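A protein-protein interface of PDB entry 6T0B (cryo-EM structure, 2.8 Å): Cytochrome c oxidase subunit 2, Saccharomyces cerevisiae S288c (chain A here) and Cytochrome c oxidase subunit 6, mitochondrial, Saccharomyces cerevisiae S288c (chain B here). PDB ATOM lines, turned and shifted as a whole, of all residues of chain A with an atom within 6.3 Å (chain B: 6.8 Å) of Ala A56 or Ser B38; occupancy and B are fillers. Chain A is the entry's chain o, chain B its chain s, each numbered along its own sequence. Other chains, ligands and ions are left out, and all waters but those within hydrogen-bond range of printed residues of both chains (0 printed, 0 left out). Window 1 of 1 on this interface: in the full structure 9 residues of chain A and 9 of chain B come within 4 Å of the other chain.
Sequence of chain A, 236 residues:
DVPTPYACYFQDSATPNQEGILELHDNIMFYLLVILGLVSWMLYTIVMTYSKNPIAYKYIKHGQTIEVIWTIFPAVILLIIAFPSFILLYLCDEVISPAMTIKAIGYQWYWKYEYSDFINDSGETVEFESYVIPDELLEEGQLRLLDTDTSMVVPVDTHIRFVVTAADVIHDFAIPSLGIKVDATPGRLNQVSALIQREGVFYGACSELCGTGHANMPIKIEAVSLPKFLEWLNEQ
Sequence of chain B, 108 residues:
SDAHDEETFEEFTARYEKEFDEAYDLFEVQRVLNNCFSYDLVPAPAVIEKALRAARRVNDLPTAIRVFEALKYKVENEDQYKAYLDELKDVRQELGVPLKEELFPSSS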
ATOM      1  N   ASN A  53      12.152 -22.583  30.267  1.00  0.00           N
ATOM      2  CA  ASN A  53      13.545 -22.310  29.969  1.00  0.00           C
ATOM      3  C   ASN A  53      14.099 -21.348  30.996  1.00  0.00           C
ATOM      4  O   ASN A  53      13.521 -20.272  31.192  1.00  0.00           O
ATOM      5  CB  ASN A  53      13.682 -21.718  28.577  1.00  0.00           C
ATOM      6  CG  ASN A  53      15.101 -21.449  28.196  1.00  0.00           C
ATOM      7  OD1 ASN A  53      16.029 -22.072  28.706  1.00  0.00           O
ATOM      8  ND2 ASN A  53      15.289 -20.504  27.290  1.00  0.00           N
ATOM      9  N   PRO A  54      15.173 -21.681  31.673  1.00  0.00           N
ATOM     10  CA  PRO A  54      15.778 -20.728  32.598  1.00  0.00           C
ATOM     11  C   PRO A  54      16.942 -19.958  32.002  1.00  0.00           C
ATOM     12  O   PRO A  54      17.491 -19.081  32.671  1.00  0.00           O
ATOM     13  CB  PRO A  54      16.235 -21.624  33.746  1.00  0.00           C
ATOM     14  CG  PRO A  54      16.578 -22.882  33.084  1.00  0.00           C
ATOM     15  CD  PRO A  54      15.670 -23.044  31.903  1.00  0.00           C
ATOM     16  N   ILE A  55      17.344 -20.257  30.769  1.00  0.00           N
ATOM     17  CA  ILE A  55      18.461 -19.568  30.126  1.00  0.00           C
ATOM     18  C   ILE A  55      17.930 -18.841  28.902  1.00  0.00           C
ATOM     19  O   ILE A  55      17.536 -19.473  27.917  1.00  0.00           O
ATOM     20  CB  ILE A  55      19.603 -20.514  29.739  1.00  0.00           C
ATOM     21  CG1 ILE A  55      20.252 -21.137  30.973  1.00  0.00           C
ATOM     22  CG2 ILE A  55      20.654 -19.766  28.959  1.00  0.00           C
ATOM     23  CD1 ILE A  55      19.756 -22.520  31.313  1.00  0.00           C
ATOM     24  N   ALA A  56      17.936 -17.516  28.957  1.00  0.00           N
ATOM     25  CA  ALA A  56      17.405 -16.684  27.892  1.00  0.00           C
ATOM     26  C   ALA A  56      18.532 -16.261  26.967  1.00  0.00           C
ATOM     27  O   ALA A  56      19.467 -15.585  27.400  1.00  0.00           O
ATOM     28  CB  ALA A  56      16.716 -15.455  28.475  1.00  0.00           C
ATOM     29  N   TYR A  57      18.419 -16.606  25.686  1.00  0.00           N
ATOM     30  CA  TYR A  57      19.426 -16.270  24.680  1.00  0.00           C
ATOM     31  C   TYR A  57      19.350 -14.771  24.427  1.00  0.00           C
ATOM     32  O   TYR A  57      18.798 -14.299  23.433  1.00  0.00           O
ATOM     33  CB  TYR A  57      19.193 -17.036  23.383  1.00  0.00           C
ATOM     34  CG  TYR A  57      19.015 -18.526  23.524  1.00  0.00           C
ATOM     35  CD1 TYR A  57      20.099 -19.374  23.463  1.00  0.00           C
ATOM     36  CD2 TYR A  57      17.758 -19.084  23.683  1.00  0.00           C
ATOM     37  CE1 TYR A  57      19.944 -20.725  23.579  1.00  0.00           C
ATOM     38  CE2 TYR A  57      17.596 -20.435  23.807  1.00  0.00           C
ATOM     39  CZ  TYR A  57      18.693 -21.250  23.753  1.00  0.00           C
ATOM     40  OH  TYR A  57      18.546 -22.610  23.873  1.00  0.00           O
ATOM     41  N   LYS A  58      19.941 -14.007  25.332  1.00  0.00           N
ATOM     42  CA  LYS A  58      19.723 -12.573  25.365  1.00  0.00           C
ATOM     43  C   LYS A  58      20.588 -11.811  24.390  1.00  0.00           C
ATOM     44  O   LYS A  58      20.675 -10.585  24.499  1.00  0.00           O
ATOM     45  CB  LYS A  58      19.945 -12.045  26.781  1.00  0.00           C
ATOM     46  CG  LYS A  58      21.306 -12.328  27.346  1.00  0.00           C
ATOM     47  CD  LYS A  58      21.461 -11.686  28.703  1.00  0.00           C
ATOM     48  CE  LYS A  58      22.821 -11.986  29.302  1.00  0.00           C
ATOM     49  NZ  LYS A  58      23.011 -11.294  30.604  1.00  0.00           N
ATOM     50  N   TYR A  59      21.230 -12.483  23.443  1.00  0.00           N
ATOM     51  CA  TYR A  59      22.047 -11.819  22.448  1.00  0.00           C
ATOM     52  C   TYR A  59      21.449 -11.897  21.060  1.00  0.00           C
ATOM     53  O   TYR A  59      22.091 -11.471  20.096  1.00  0.00           O
ATOM     54  CB  TYR A  59      23.449 -12.414  22.445  1.00  0.00           C
ATOM     55  CG  TYR A  59      24.216 -12.058  23.680  1.00  0.00           C
ATOM     56  CD1 TYR A  59      24.219 -10.763  24.160  1.00  0.00           C
ATOM     57  CD2 TYR A  59      24.919 -13.018  24.379  1.00  0.00           C
ATOM     58  CE1 TYR A  59      24.915 -10.429  25.295  1.00  0.00           C
ATOM     59  CE2 TYR A  59      25.618 -12.698  25.510  1.00  0.00           C
ATOM     60  CZ  TYR A  59      25.612 -11.402  25.967  1.00  0.00           C
ATOM     61  OH  TYR A  59      26.312 -11.078  27.104  1.00  0.00           O
ATOM     62  N   TYR B  16      36.079 -17.167  25.522  1.00  0.00           N
ATOM     63  CA  TYR B  16      35.596 -17.400  26.875  1.00  0.00           C
ATOM     64  C   TYR B  16      36.617 -18.119  27.739  1.00  0.00           C
ATOM     65  O   TYR B  16      36.570 -17.978  28.965  1.00  0.00           O
ATOM     66  CB  TYR B  16      34.282 -18.161  26.851  1.00  0.00           C
ATOM     67  CG  TYR B  16      33.129 -17.216  26.827  1.00  0.00           C
ATOM     68  CD1 TYR B  16      32.871 -16.399  27.904  1.00  0.00           C
ATOM     69  CD2 TYR B  16      32.333 -17.098  25.715  1.00  0.00           C
ATOM     70  CE1 TYR B  16      31.833 -15.512  27.885  1.00  0.00           C
ATOM     71  CE2 TYR B  16      31.294 -16.211  25.685  1.00  0.00           C
ATOM     72  CZ  TYR B  16      31.047 -15.423  26.772  1.00  0.00           C
ATOM     73  OH  TYR B  16      30.000 -14.535  26.739  1.00  0.00           O
ATOM     74  N   LEU B  33      29.729 -16.870  33.262  1.00  0.00           N
ATOM     75  CA  LEU B  33      29.042 -18.120  32.965  1.00  0.00           C
ATOM     76  C   LEU B  33      27.685 -17.859  32.332  1.00  0.00           C
ATOM     77  O   LEU B  33      27.290 -18.569  31.403  1.00  0.00           O
ATOM     78  CB  LEU B  33      28.878 -18.932  34.238  1.00  0.00           C
ATOM     79  CG  LEU B  33      28.762 -20.443  34.172  1.00  0.00           C
ATOM     80  CD1 LEU B  33      29.123 -20.894  35.526  1.00  0.00           C
ATOM     81  CD2 LEU B  33      27.450 -20.970  33.782  1.00  0.00           C
ATOM     82  N   ASN B  34      26.945 -16.883  32.859  1.00  0.00           N
ATOM     83  CA  ASN B  34      25.647 -16.530  32.298  1.00  0.00           C
ATOM     84  C   ASN B  34      25.795 -16.035  30.871  1.00  0.00           C
ATOM     85  O   ASN B  34      25.026 -16.430  29.980  1.00  0.00           O
ATOM     86  CB  ASN B  34      24.979 -15.468  33.166  1.00  0.00           C
ATOM     87  CG  ASN B  34      23.521 -15.303  32.854  1.00  0.00           C
ATOM     88  OD1 ASN B  34      22.799 -16.281  32.692  1.00  0.00           O
ATOM     89  ND2 ASN B  34      23.069 -14.062  32.774  1.00  0.00           N
ATOM     90  N   ASN B  35      26.838 -15.244  30.620  1.00  0.00           N
ATOM     91  CA  ASN B  35      27.081 -14.740  29.280  1.00  0.00           C
ATOM     92  C   ASN B  35      27.531 -15.833  28.320  1.00  0.00           C
ATOM     93  O   ASN B  35      27.209 -15.763  27.133  1.00  0.00           O
ATOM     94  CB  ASN B  35      28.103 -13.613  29.328  1.00  0.00           C
ATOM     95  CG  ASN B  35      27.501 -12.323  29.800  1.00  0.00           C
ATOM     96  OD1 ASN B  35      26.312 -12.076  29.604  1.00  0.00           O
ATOM     97  ND2 ASN B  35      28.313 -11.484  30.431  1.00  0.00           N
ATOM     98  N   CYS B  36      28.250 -16.854  28.792  1.00  0.00           N
ATOM     99  CA  CYS B  36      28.677 -17.882  27.848  1.00  0.00           C
ATOM    100  C   CYS B  36      27.614 -18.941  27.636  1.00  0.00           C
ATOM    101  O   CYS B  36      27.611 -19.601  26.592  1.00  0.00           O
ATOM    102  CB  CYS B  36      29.973 -18.552  28.292  1.00  0.00           C
ATOM    103  SG  CYS B  36      29.841 -19.633  29.713  1.00  0.00           S
ATOM    104  N   PHE B  37      26.713 -19.138  28.597  1.00  0.00           N
ATOM    105  CA  PHE B  37      25.666 -20.126  28.389  1.00  0.00           C
ATOM    106  C   PHE B  37      24.449 -19.548  27.707  1.00  0.00           C
ATOM    107  O   PHE B  37      23.638 -20.309  27.179  1.00  0.00           O
ATOM    108  CB  PHE B  37      25.243 -20.770  29.704  1.00  0.00           C
ATOM    109  CG  PHE B  37      25.953 -22.036  29.983  1.00  0.00           C
ATOM    110  CD1 PHE B  37      27.270 -22.008  30.381  1.00  0.00           C
ATOM    111  CD2 PHE B  37      25.321 -23.258  29.841  1.00  0.00           C
ATOM    112  CE1 PHE B  37      27.945 -23.170  30.624  1.00  0.00           C
ATOM    113  CE2 PHE B  37      26.000 -24.416  30.081  1.00  0.00           C
ATOM    114  CZ  PHE B  37      27.318 -24.363  30.480  1.00  0.00           C
ATOM    115  N   SER B  38      24.295 -18.233  27.685  1.00  0.00           N
ATOM    116  CA  SER B  38      23.152 -17.709  26.959  1.00  0.00           C
ATOM    117  C   SER B  38      23.500 -17.396  25.513  1.00  0.00           C
ATOM    118  O   SER B  38      23.187 -16.328  24.992  1.00  0.00           O
ATOM    119  CB  SER B  38      22.605 -16.488  27.677  1.00  0.00           C
ATOM    120  OG  SER B  38      23.597 -15.494  27.791  1.00  0.00           O
ATOM    121  N   TYR B  39      24.126 -18.359  24.844  1.00  0.00           N
ATOM    122  CA  TYR B  39      24.328 -18.357  23.406  1.00  0.00           C
ATOM    123  C   TYR B  39      23.619 -19.569  22.820  1.00  0.00           C
ATOM    124  O   TYR B  39      23.138 -20.439  23.549  1.00  0.00           O
ATOM    125  CB  TYR B  39      25.815 -18.379  23.048  1.00  0.00           C
ATOM    126  CG  TYR B  39      26.445 -17.012  23.020  1.00  0.00           C
ATOM    127  CD1 TYR B  39      26.241 -16.157  21.956  1.00  0.00           C
ATOM    128  CD2 TYR B  39      27.240 -16.579  24.059  1.00  0.00           C
ATOM    129  CE1 TYR B  39      26.813 -14.906  21.932  1.00  0.00           C
ATOM    130  CE2 TYR B  39      27.814 -15.333  24.046  1.00  0.00           C
ATOM    131  CZ  TYR B  39      27.604 -14.504  22.981  1.00  0.00           C
ATOM    132  OH  TYR B  39      28.178 -13.257  22.968  1.00  0.00           O
ATOM    133  N   ASP B  40      23.550 -19.598  21.486  1.00  0.00           N
ATOM    134  CA  ASP B  40      22.858 -20.670  20.770  1.00  0.00           C
ATOM    135  C   ASP B  40      23.518 -22.019  21.023  1.00  0.00           C
ATOM    136  O   ASP B  40      22.841 -23.035  21.202  1.00  0.00           O
ATOM    137  CB  ASP B  40      22.859 -20.355  19.274  1.00  0.00           C
ATOM    138  CG  ASP B  40      21.768 -21.078  18.505  1.00  0.00           C
ATOM    139  OD1 ASP B  40      21.574 -22.300  18.686  1.00  0.00           O
ATOM    140  OD2 ASP B  40      21.101 -20.412  17.691  1.00  0.00           O
ATOM    141  N   LEU B  41      24.836 -22.037  21.054  1.00  0.00           N
ATOM    142  CA  LEU B  41      25.590 -23.271  21.095  1.00  0.00           C
ATOM    143  C   LEU B  41      26.097 -23.547  22.500  1.00  0.00           C
ATOM    144  O   LEU B  41      26.466 -22.629  23.235  1.00  0.00           O
ATOM    145  CB  LEU B  41      26.752 -23.207  20.107  1.00  0.00           C
ATOM    146  CG  LEU B  41      28.007 -22.371  20.347  1.00  0.00           C
ATOM    147  CD1 LEU B  41      29.014 -22.816  19.344  1.00  0.00           C
ATOM    148  CD2 LEU B  41      27.789 -20.885  20.183  1.00  0.00           C
ATOM    149  N   LYS B  74      21.346 -27.600  28.612  1.00  0.00           N
ATOM    150  CA  LYS B  74      21.758 -27.058  27.323  1.00  0.00           C
ATOM    151  C   LYS B  74      21.875 -28.112  26.222  1.00  0.00           C
ATOM    152  O   LYS B  74      21.536 -27.823  25.070  1.00  0.00           O
ATOM    153  CB  LYS B  74      23.082 -26.326  27.471  1.00  0.00           C
ATOM    154  CG  LYS B  74      23.295 -25.290  26.417  1.00  0.00           C
ATOM    155  CD  LYS B  74      22.401 -24.111  26.659  1.00  0.00           C
ATOM    156  CE  LYS B  74      22.535 -23.107  25.550  1.00  0.00           C
ATOM    157  NZ  LYS B  74      21.923 -21.824  25.946  1.00  0.00           N
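The side-chain hydroxyl of Tyr A59 is in hydrogen-bond range of the side-chain amide oxygen of Asn B35 (2.7 Å).
Ala A56 touches one residue of chain B. Of chain A, only Ile A55 (3.8 Å), Ala A56 (3.3 Å), Tyr A57 (3.8 Å), Lys A58 (3.9 Å) and Tyr A59 (3.8 Å) come within 4 Å of Ser B38. Printed residues of chain A within 4 Å of Asn B35: Lys A58 (3.5 Å) and Tyr A59 (2.7 Å). Of the printed residues of chain A, Lys B74 touches Ile A55 (3.9 Å) and Tyr A57 (3.3 Å). Of the printed residues of chain A, Phe B37 touches Ile A55 (3.5 Å). Of the printed residues of chain A, Tyr B39 touches Tyr A57 (3.2 Å) and Tyr A59 (3.4 Å). Asn A53 touches none of the printed residues of chain B. Pro A54 touches none of the printed residues of chain B.
The side-chain amide nitrogen of Asn A53 sits at hydrogen-bond distance from the backbone carbonyl oxygen of Ile A55. OH of Tyr B16 is in hydrogen-bond range of O of Asn B35, at 3.1 Å. The side-chain hydroxyl (OG) of Ser B38 is in hydrogen-bond range of the backbone carbonyl oxygen (O) of Asn B34, at 2.8 Å. The backbone carbonyl oxygen (O) of Phe B37 lies within hydrogen-bond range of the side-chain amino group (NZ) of Lys B74. The side-chain amino group (NZ) of Lys B74 sits at hydrogen-bond distance from the backbone carbonyl oxygen (O) of Tyr B39, at 3.0 Å.
Among the printed residues, merely in contact across the chains: Ile A55 with Phe B37 (3.5 Å), Ile A55 with Ser B38 (3.8 Å), Ile A55 with Lys B74 (3.9 Å), Ala A56 with Ser B38 (3.3 Å), Tyr A57 with Ser B38 (3.8 Å), Tyr A57 with Tyr B39 (3.2 Å), Tyr A57 with Asp B40 (3.98 Å), Tyr A57 with Lys B74 (3.3 Å), Lys A58 with Asn B34 (3.5 Å), Lys A58 with Asn B35 (3.5 Å), Lys A58 with Ser B38 (3.9 Å), Tyr A59 with Ser B38 (3.8 Å) and Tyr A59 with Tyr B39 (3.4 Å).
Of the 11 printed residues of chain B, 7 touch a printed residue of chain A. Among the printed residues, 14 pairs touch across the chains.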
